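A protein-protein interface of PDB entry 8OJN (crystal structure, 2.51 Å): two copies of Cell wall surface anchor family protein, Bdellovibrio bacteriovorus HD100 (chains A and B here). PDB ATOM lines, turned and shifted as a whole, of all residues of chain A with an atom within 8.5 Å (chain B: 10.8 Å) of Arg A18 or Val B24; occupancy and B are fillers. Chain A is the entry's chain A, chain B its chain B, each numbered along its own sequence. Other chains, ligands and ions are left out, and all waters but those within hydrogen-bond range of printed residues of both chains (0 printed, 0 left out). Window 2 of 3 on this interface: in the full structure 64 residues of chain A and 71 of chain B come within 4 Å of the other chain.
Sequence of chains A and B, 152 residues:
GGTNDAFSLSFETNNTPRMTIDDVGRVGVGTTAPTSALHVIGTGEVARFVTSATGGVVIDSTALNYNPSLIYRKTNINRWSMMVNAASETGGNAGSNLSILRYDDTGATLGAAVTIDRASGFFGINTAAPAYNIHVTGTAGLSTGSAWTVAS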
ATOM      1  N   ARG A  18       2.875  10.965   4.778  1.00  0.00           N
ATOM      2  CA  ARG A  18       2.083  10.100   5.639  1.00  0.00           C
ATOM      3  C   ARG A  18       0.582  10.065   5.276  1.00  0.00           C
ATOM      4  O   ARG A  18       0.104   9.003   4.879  1.00  0.00           O
ATOM      5  CB  ARG A  18       2.291  10.486   7.105  1.00  0.00           C
ATOM      6  CG  ARG A  18       3.718  10.176   7.589  1.00  0.00           C
ATOM      7  CD  ARG A  18       3.864   8.847   8.376  1.00  0.00           C
ATOM      8  NE  ARG A  18       5.218   8.585   8.903  1.00  0.00           N
ATOM      9  CZ  ARG A  18       5.816   9.313   9.849  1.00  0.00           C
ATOM     10  NH1 ARG A  18       5.204  10.364  10.365  1.00  0.00           N
ATOM     11  NH2 ARG A  18       7.042   8.999  10.267  1.00  0.00           N
ATOM     12  N   MET A  19      -0.182  11.154   5.394  1.00  0.00           N
ATOM     13  CA  MET A  19      -1.584  11.062   4.985  1.00  0.00           C
ATOM     14  C   MET A  19      -1.728  11.275   3.479  1.00  0.00           C
ATOM     15  O   MET A  19      -1.135  12.193   2.904  1.00  0.00           O
ATOM     16  CB  MET A  19      -2.491  12.042   5.728  1.00  0.00           C
ATOM     17  CG  MET A  19      -3.940  11.901   5.234  1.00  0.00           C
ATOM     18  SD  MET A  19      -4.595  13.332   4.350  1.00  0.00           S
ATOM     19  CE  MET A  19      -5.652  14.029   5.608  1.00  0.00           C
ATOM     20  N   THR A  20      -2.547  10.420   2.857  1.00  0.00           N
ATOM     21  CA  THR A  20      -2.631  10.256   1.410  1.00  0.00           C
ATOM     22  C   THR A  20      -4.083  10.044   0.999  1.00  0.00           C
ATOM     23  O   THR A  20      -4.825   9.344   1.689  1.00  0.00           O
ATOM     24  CB  THR A  20      -1.780   9.052   0.960  1.00  0.00           C
ATOM     25  OG1 THR A  20      -0.398   9.298   1.249  1.00  0.00           O
ATOM     26  CG2 THR A  20      -1.944   8.770  -0.527  1.00  0.00           C
ATOM     27  N   ILE A  21      -4.489  10.629  -0.124  1.00  0.00           N
ATOM     28  CA  ILE A  21      -5.862  10.502  -0.631  1.00  0.00           C
ATOM     29  C   ILE A  21      -5.770   9.936  -2.047  1.00  0.00           C
ATOM     30  O   ILE A  21      -5.582  10.679  -3.013  1.00  0.00           O
ATOM     31  CB  ILE A  21      -6.613  11.835  -0.617  1.00  0.00           C
ATOM     32  CG1 ILE A  21      -6.547  12.480   0.773  1.00  0.00           C
ATOM     33  CG2 ILE A  21      -8.047  11.633  -1.075  1.00  0.00           C
ATOM     34  CD1 ILE A  21      -7.582  13.561   1.001  1.00  0.00           C
ATOM     35  N   VAL A  27      -8.669   7.038   1.829  1.00  0.00           N
ATOM     36  CA  VAL A  27      -7.814   7.877   2.657  1.00  0.00           C
ATOM     37  C   VAL A  27      -6.913   6.974   3.485  1.00  0.00           C
ATOM     38  O   VAL A  27      -7.399   6.179   4.300  1.00  0.00           O
ATOM     39  CB  VAL A  27      -8.641   8.802   3.562  1.00  0.00           C
ATOM     40  CG1 VAL A  27      -7.732   9.552   4.532  1.00  0.00           C
ATOM     41  CG2 VAL A  27      -9.456   9.767   2.721  1.00  0.00           C
ATOM     42  N   GLY A  28      -5.607   7.099   3.283  1.00  0.00           N
ATOM     43  CA  GLY A  28      -4.643   6.385   4.088  1.00  0.00           C
ATOM     44  C   GLY A  28      -3.911   7.297   5.048  1.00  0.00           C
ATOM     45  O   GLY A  28      -3.201   8.216   4.628  1.00  0.00           O
ATOM     46  N   VAL A  29      -4.091   7.060   6.341  1.00  0.00           N
ATOM     47  CA  VAL A  29      -3.331   7.745   7.379  1.00  0.00           C
ATOM     48  C   VAL A  29      -2.129   6.877   7.734  1.00  0.00           C
ATOM     49  O   VAL A  29      -2.286   5.741   8.197  1.00  0.00           O
ATOM     50  CB  VAL A  29      -4.200   8.021   8.613  1.00  0.00           C
ATOM     51  CG1 VAL A  29      -3.369   8.654   9.722  1.00  0.00           C
ATOM     52  CG2 VAL A  29      -5.372   8.905   8.241  1.00  0.00           C
ATOM     53  N   GLY A  30      -0.928   7.403   7.507  1.00  0.00           N
ATOM     54  CA  GLY A  30       0.283   6.653   7.756  1.00  0.00           C
ATOM     55  C   GLY A  30       0.674   5.671   6.672  1.00  0.00           C
ATOM     56  O   GLY A  30       1.715   5.017   6.803  1.00  0.00           O
ATOM     57  N   THR A  31      -0.124   5.540   5.611  1.00  0.00           N
ATOM     58  CA  THR A  31       0.206   4.672   4.488  1.00  0.00           C
ATOM     59  C   THR A  31      -0.166   5.354   3.181  1.00  0.00           C
ATOM     60  O   THR A  31      -1.086   6.174   3.127  1.00  0.00           O
ATOM     61  CB  THR A  31      -0.509   3.312   4.562  1.00  0.00           C
ATOM     62  OG1 THR A  31      -0.224   2.561   3.375  1.00  0.00           O
ATOM     63  CG2 THR A  31      -2.017   3.492   4.686  1.00  0.00           C
ATOM     64  N   THR A  32       0.562   4.992   2.125  1.00  0.00           N
ATOM     65  CA  THR A  32       0.349   5.522   0.785  1.00  0.00           C
ATOM     66  C   THR A  32      -0.517   4.621  -0.085  1.00  0.00           C
ATOM     67  O   THR A  32      -1.020   5.077  -1.118  1.00  0.00           O
ATOM     68  CB  THR A  32       1.701   5.737   0.091  1.00  0.00           C
ATOM     69  OG1 THR A  32       2.662   6.164   1.063  1.00  0.00           O
ATOM     70  CG2 THR A  32       1.590   6.788  -1.021  1.00  0.00           C
ATOM     71  N   ALA A  33      -0.712   3.360   0.309  1.00  0.00           N
ATOM     72  CA  ALA A  33      -1.486   2.386  -0.456  1.00  0.00           C
ATOM     73  C   ALA A  33      -2.645   1.888   0.400  1.00  0.00           C
ATOM     74  O   ALA A  33      -2.622   0.755   0.904  1.00  0.00           O
ATOM     75  CB  ALA A  33      -0.608   1.224  -0.919  1.00  0.00           C
ATOM     76  N   PRO A  34      -3.680   2.710   0.583  1.00  0.00           N
ATOM     77  CA  PRO A  34      -4.813   2.295   1.419  1.00  0.00           C
ATOM     78  C   PRO A  34      -5.687   1.288   0.682  1.00  0.00           C
ATOM     79  O   PRO A  34      -6.049   1.490  -0.479  1.00  0.00           O
ATOM     80  CB  PRO A  34      -5.561   3.606   1.678  1.00  0.00           C
ATOM     81  CG  PRO A  34      -5.261   4.442   0.465  1.00  0.00           C
ATOM     82  CD  PRO A  34      -3.875   4.055   0.008  1.00  0.00           C
ATOM     83  N   HIS A  39      -7.853   3.831   5.933  1.00  0.00           N
ATOM     84  CA  HIS A  39      -6.815   2.861   6.280  1.00  0.00           C
ATOM     85  C   HIS A  39      -5.786   3.574   7.152  1.00  0.00           C
ATOM     86  O   HIS A  39      -4.977   4.357   6.649  1.00  0.00           O
ATOM     87  CB  HIS A  39      -6.186   2.276   5.018  1.00  0.00           C
ATOM     88  CG  HIS A  39      -5.200   1.178   5.272  1.00  0.00           C
ATOM     89  ND1 HIS A  39      -4.574   0.494   4.252  1.00  0.00           N
ATOM     90  CD2 HIS A  39      -4.728   0.647   6.425  1.00  0.00           C
ATOM     91  CE1 HIS A  39      -3.758  -0.409   4.765  1.00  0.00           C
ATOM     92  NE2 HIS A  39      -3.834  -0.338   6.082  1.00  0.00           N
ATOM     93  N   VAL A  40      -5.810   3.307   8.455  1.00  0.00           N
ATOM     94  CA  VAL A  40      -4.949   3.992   9.414  1.00  0.00           C
ATOM     95  C   VAL A  40      -3.909   3.014   9.942  1.00  0.00           C
ATOM     96  O   VAL A  40      -4.226   1.861  10.256  1.00  0.00           O
ATOM     97  CB  VAL A  40      -5.768   4.600  10.570  1.00  0.00           C
ATOM     98  CG1 VAL A  40      -4.880   5.474  11.456  1.00  0.00           C
ATOM     99  CG2 VAL A  40      -6.943   5.395  10.016  1.00  0.00           C
ATOM    100  N   ILE A  41      -2.669   3.482  10.045  1.00  0.00           N
ATOM    101  CA  ILE A  41      -1.542   2.675  10.501  1.00  0.00           C
ATOM    102  C   ILE A  41      -0.913   3.369  11.701  1.00  0.00           C
ATOM    103  O   ILE A  41      -0.649   4.577  11.658  1.00  0.00           O
ATOM    104  CB  ILE A  41      -0.510   2.466   9.375  1.00  0.00           C
ATOM    105  CG1 ILE A  41      -0.890   1.246   8.534  1.00  0.00           C
ATOM    106  CG2 ILE A  41       0.901   2.333   9.935  1.00  0.00           C
ATOM    107  CD1 ILE A  41      -0.018   1.056   7.317  1.00  0.00           C
ATOM    108  N   THR B  20      -6.512  18.836  12.121  1.00  0.00           N
ATOM    109  CA  THR B  20      -5.112  19.201  11.964  1.00  0.00           C
ATOM    110  C   THR B  20      -4.263  17.971  11.664  1.00  0.00           C
ATOM    111  O   THR B  20      -4.683  16.827  11.859  1.00  0.00           O
ATOM    112  CB  THR B  20      -4.563  19.905  13.219  1.00  0.00           C
ATOM    113  OG1 THR B  20      -4.445  18.957  14.287  1.00  0.00           O
ATOM    114  CG2 THR B  20      -5.480  21.042  13.660  1.00  0.00           C
ATOM    115  N   ILE B  21      -3.053  18.231  11.176  1.00  0.00           N
ATOM    116  CA  ILE B  21      -2.022  17.219  10.972  1.00  0.00           C
ATOM    117  C   ILE B  21      -0.727  17.777  11.537  1.00  0.00           C
ATOM    118  O   ILE B  21      -0.369  18.923  11.242  1.00  0.00           O
ATOM    119  CB  ILE B  21      -1.860  16.864   9.483  1.00  0.00           C
ATOM    120  CG1 ILE B  21      -3.224  16.586   8.862  1.00  0.00           C
ATOM    121  CG2 ILE B  21      -0.924  15.684   9.308  1.00  0.00           C
ATOM    122  CD1 ILE B  21      -3.165  15.815   7.593  1.00  0.00           C
ATOM    123  N   ASP B  22      -0.028  16.989  12.354  1.00  0.00           N
ATOM    124  CA  ASP B  22       1.108  17.521  13.096  1.00  0.00           C
ATOM    125  C   ASP B  22       2.421  16.911  12.604  1.00  0.00           C
ATOM    126  O   ASP B  22       2.450  16.095  11.677  1.00  0.00           O
ATOM    127  CB  ASP B  22       0.915  17.313  14.604  1.00  0.00           C
ATOM    128  CG  ASP B  22       0.910  15.845  15.018  1.00  0.00           C
ATOM    129  OD1 ASP B  22       1.082  14.961  14.156  1.00  0.00           O
ATOM    130  OD2 ASP B  22       0.735  15.573  16.225  1.00  0.00           O
ATOM    131  N   ASP B  23       3.512  17.337  13.252  1.00  0.00           N
ATOM    132  CA  ASP B  23       4.869  16.876  12.957  1.00  0.00           C
ATOM    133  C   ASP B  23       4.949  15.372  12.695  1.00  0.00           C
ATOM    134  O   ASP B  23       5.470  14.934  11.663  1.00  0.00           O
ATOM    135  CB  ASP B  23       5.775  17.270  14.133  1.00  0.00           C
ATOM    136  CG  ASP B  23       7.247  16.915  13.917  1.00  0.00           C
ATOM    137  OD1 ASP B  23       7.599  16.168  12.978  1.00  0.00           O
ATOM    138  OD2 ASP B  23       8.070  17.397  14.725  1.00  0.00           O
ATOM    139  N   VAL B  24       4.411  14.597  13.644  1.00  0.00           N
ATOM    140  CA  VAL B  24       4.405  13.104  13.592  1.00  0.00           C
ATOM    141  C   VAL B  24       3.322  12.623  12.617  1.00  0.00           C
ATOM    142  O   VAL B  24       3.107  11.399  12.535  1.00  0.00           O
ATOM    143  CB  VAL B  24       4.195  12.505  14.996  1.00  0.00           C
ATOM    144  CG1 VAL B  24       4.375  10.994  14.997  1.00  0.00           C
ATOM    145  CG2 VAL B  24       5.104  13.155  16.026  1.00  0.00           C
ATOM    146  N   GLY B  25       2.692  13.554  11.895  1.00  0.00           N
ATOM    147  CA  GLY B  25       1.645  13.223  10.908  1.00  0.00           C
ATOM    148  C   GLY B  25       0.452  12.484  11.497  1.00  0.00           C
ATOM    149  O   GLY B  25      -0.013  11.523  10.856  1.00  0.00           O
ATOM    150  N   ARG B  26       0.001  12.879  12.692  1.00  0.00           N
ATOM    151  CA  ARG B  26      -1.202  12.266  13.319  1.00  0.00           C
ATOM    152  C   ARG B  26      -2.403  13.140  12.940  1.00  0.00           C
ATOM    153  O   ARG B  26      -2.297  14.366  13.126  1.00  0.00           O
ATOM    154  CB  ARG B  26      -1.077  12.275  14.845  1.00  0.00           C
ATOM    155  CG  ARG B  26       0.144  11.557  15.398  1.00  0.00           C
ATOM    156  CD  ARG B  26       0.192  11.718  16.905  1.00  0.00           C
ATOM    157  NE  ARG B  26       1.420  11.213  17.500  1.00  0.00           N
ATOM    158  CZ  ARG B  26       1.753  11.368  18.775  1.00  0.00           C
ATOM    159  NH1 ARG B  26       0.947  12.020  19.596  1.00  0.00           N
ATOM    160  NH2 ARG B  26       2.892  10.872  19.227  1.00  0.00           N
ATOM    161  N   VAL B  27      -3.502  12.553  12.453  1.00  0.00           N
ATOM    162  CA  VAL B  27      -4.622  13.407  12.078  1.00  0.00           C
ATOM    163  C   VAL B  27      -5.598  13.494  13.247  1.00  0.00           C
ATOM    164  O   VAL B  27      -6.007  12.469  13.806  1.00  0.00           O
ATOM    165  CB  VAL B  27      -5.311  12.879  10.812  1.00  0.00           C
ATOM    166  CG1 VAL B  27      -6.546  13.707  10.496  1.00  0.00           C
ATOM    167  CG2 VAL B  27      -4.331  12.899   9.647  1.00  0.00           C
ATOM    168  N   GLY B  28      -5.965  14.710  13.622  1.00  0.00           N
ATOM    169  CA  GLY B  28      -6.927  14.941  14.692  1.00  0.00           C
ATOM    170  C   GLY B  28      -8.156  15.657  14.169  1.00  0.00           C
ATOM    171  O   GLY B  28      -8.043  16.608  13.397  1.00  0.00           O
ATOM    172  N   THR B  32      -6.832  19.592  18.439  1.00  0.00           N
ATOM    173  CA  THR B  32      -5.594  20.053  17.833  1.00  0.00           C
ATOM    174  C   THR B  32      -4.369  19.411  18.468  1.00  0.00           C
ATOM    175  O   THR B  32      -3.241  19.734  18.077  1.00  0.00           O
ATOM    176  CB  THR B  32      -5.482  21.583  17.907  1.00  0.00           C
ATOM    177  OG1 THR B  32      -4.242  22.000  17.319  1.00  0.00           O
ATOM    178  CG2 THR B  32      -5.550  22.064  19.352  1.00  0.00           C
ATOM    179  N   ALA B  33      -4.562  18.509  19.432  1.00  0.00           N
ATOM    180  CA  ALA B  33      -3.489  17.743  20.059  1.00  0.00           C
ATOM    181  C   ALA B  33      -3.781  16.265  19.827  1.00  0.00           C
ATOM    182  O   ALA B  33      -4.279  15.568  20.727  1.00  0.00           O
ATOM    183  CB  ALA B  33      -3.368  18.061  21.549  1.00  0.00           C
ATOM    184  N   PRO B  34      -3.500  15.753  18.629  1.00  0.00           N
ATOM    185  CA  PRO B  34      -3.743  14.328  18.366  1.00  0.00           C
ATOM    186  C   PRO B  34      -2.731  13.476  19.117  1.00  0.00           C
ATOM    187  O   PRO B  34      -1.533  13.762  19.104  1.00  0.00           O
ATOM    188  CB  PRO B  34      -3.570  14.204  16.845  1.00  0.00           C
ATOM    189  CG  PRO B  34      -3.429  15.618  16.326  1.00  0.00           C
ATOM    190  CD  PRO B  34      -2.916  16.433  17.462  1.00  0.00           C
ATOM    191  N   THR B  35      -3.227  12.430  19.785  1.00  0.00           N
ATOM    192  CA  THR B  35      -2.375  11.504  20.521  1.00  0.00           C
ATOM    193  C   THR B  35      -2.267  10.130  19.869  1.00  0.00           C
ATOM    194  O   THR B  35      -1.452   9.313  20.316  1.00  0.00           O
ATOM    195  CB  THR B  35      -2.880  11.341  21.963  1.00  0.00           C
ATOM    196  OG1 THR B  35      -4.076  10.552  21.968  1.00  0.00           O
ATOM    197  CG2 THR B  35      -3.172  12.702  22.575  1.00  0.00           C
ATOM    198  N   SER B  36      -3.061   9.856  18.836  1.00  0.00           N
ATOM    199  CA  SER B  36      -2.988   8.629  18.056  1.00  0.00           C
ATOM    200  C   SER B  36      -2.882   8.992  16.581  1.00  0.00           C
ATOM    201  O   SER B  36      -3.034  10.155  16.199  1.00  0.00           O
ATOM    202  CB  SER B  36      -4.212   7.737  18.294  1.00  0.00           C
ATOM    203  OG  SER B  36      -4.621   7.800  19.644  1.00  0.00           O
ATOM    204  N   ALA B  37      -2.626   7.977  15.748  1.00  0.00           N
ATOM    205  CA  ALA B  37      -2.560   8.204  14.306  1.00  0.00           C
ATOM    206  C   ALA B  37      -3.839   8.860  13.793  1.00  0.00           C
ATOM    207  O   ALA B  37      -3.795   9.718  12.905  1.00  0.00           O
ATOM    208  CB  ALA B  37      -2.295   6.887  13.578  1.00  0.00           C
ATOM    209  N   LEU B  38      -4.984   8.469  14.349  1.00  0.00           N
ATOM    210  CA  LEU B  38      -6.256   9.138  14.122  1.00  0.00           C
ATOM    211  C   LEU B  38      -6.867   9.451  15.477  1.00  0.00           C
ATOM    212  O   LEU B  38      -6.911   8.585  16.354  1.00  0.00           O
ATOM    213  CB  LEU B  38      -7.217   8.274  13.295  1.00  0.00           C
ATOM    214  CG  LEU B  38      -8.515   8.958  12.859  1.00  0.00           C
ATOM    215  CD1 LEU B  38      -8.200  10.218  12.059  1.00  0.00           C
ATOM    216  CD2 LEU B  38      -9.399   8.010  12.051  1.00  0.00           C
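The backbone carbonyl oxygen of Val B24 sits at hydrogen-bond distance from the guanidinium group of Arg A18.
N of Val B24 sits close to OD1 of Asp B22 (3.4 Å). The backbone carbonyl oxygen (O) of Ala B37 sits at hydrogen-bond distance from the backbone NH (N) of Val B27, at 2.9 Å. The backbone carbonyl oxygen (O) of Arg A18 lies within hydrogen-bond range of the backbone NH (N) of Gly A30 (3.2 Å). O of His A39 is in hydrogen-bond range of N of Val A29 (2.9 Å). O of Val A29 is in hydrogen-bond range of N of Ile A41.
CD1 of Ile B21 touches CE of Met A19 (3.6 Å). Val A29 touches Ala B37. Val A40 touches Ala B37. Ile A41 touches Ala B37.
Of chain B, only Val B24 comes within 4 Å of Arg A18. Of the printed residues of chain B, Met A19 touches Ile B21 (3.6 Å). No residue of chain B comes within 4 Å of Thr A20. No residue of chain B comes within 4 Å of Gly A28. No residue of chain B comes within 4 Å of Gly A30. Printed residues of chain B within 4 Å of Val A40: Ala B37 (3.6 Å). Val B24 touches one residue of chain A. The nearest printed residue of chain B that does not touch Val A40 is Leu B38 (4.1 Å).
Hydrophobic or aromatic side chains of chain B within 4 Å of the printed part of chain A: Ile B21 and Ala B37. Of the 15 printed residues of chain A, 5 touch a printed residue of chain B. Among the printed residues, no Asp or Glu carboxylate lies within 4 Å of a Lys or Arg side-chain nitrogen of the other chain.
Positions printed for both chains: 20, 21, 27, 28, 32, 33 and 34. Of the 5 pairs that touch across the chains among the printed residues, none has its exchanged pair printed and touching as well.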
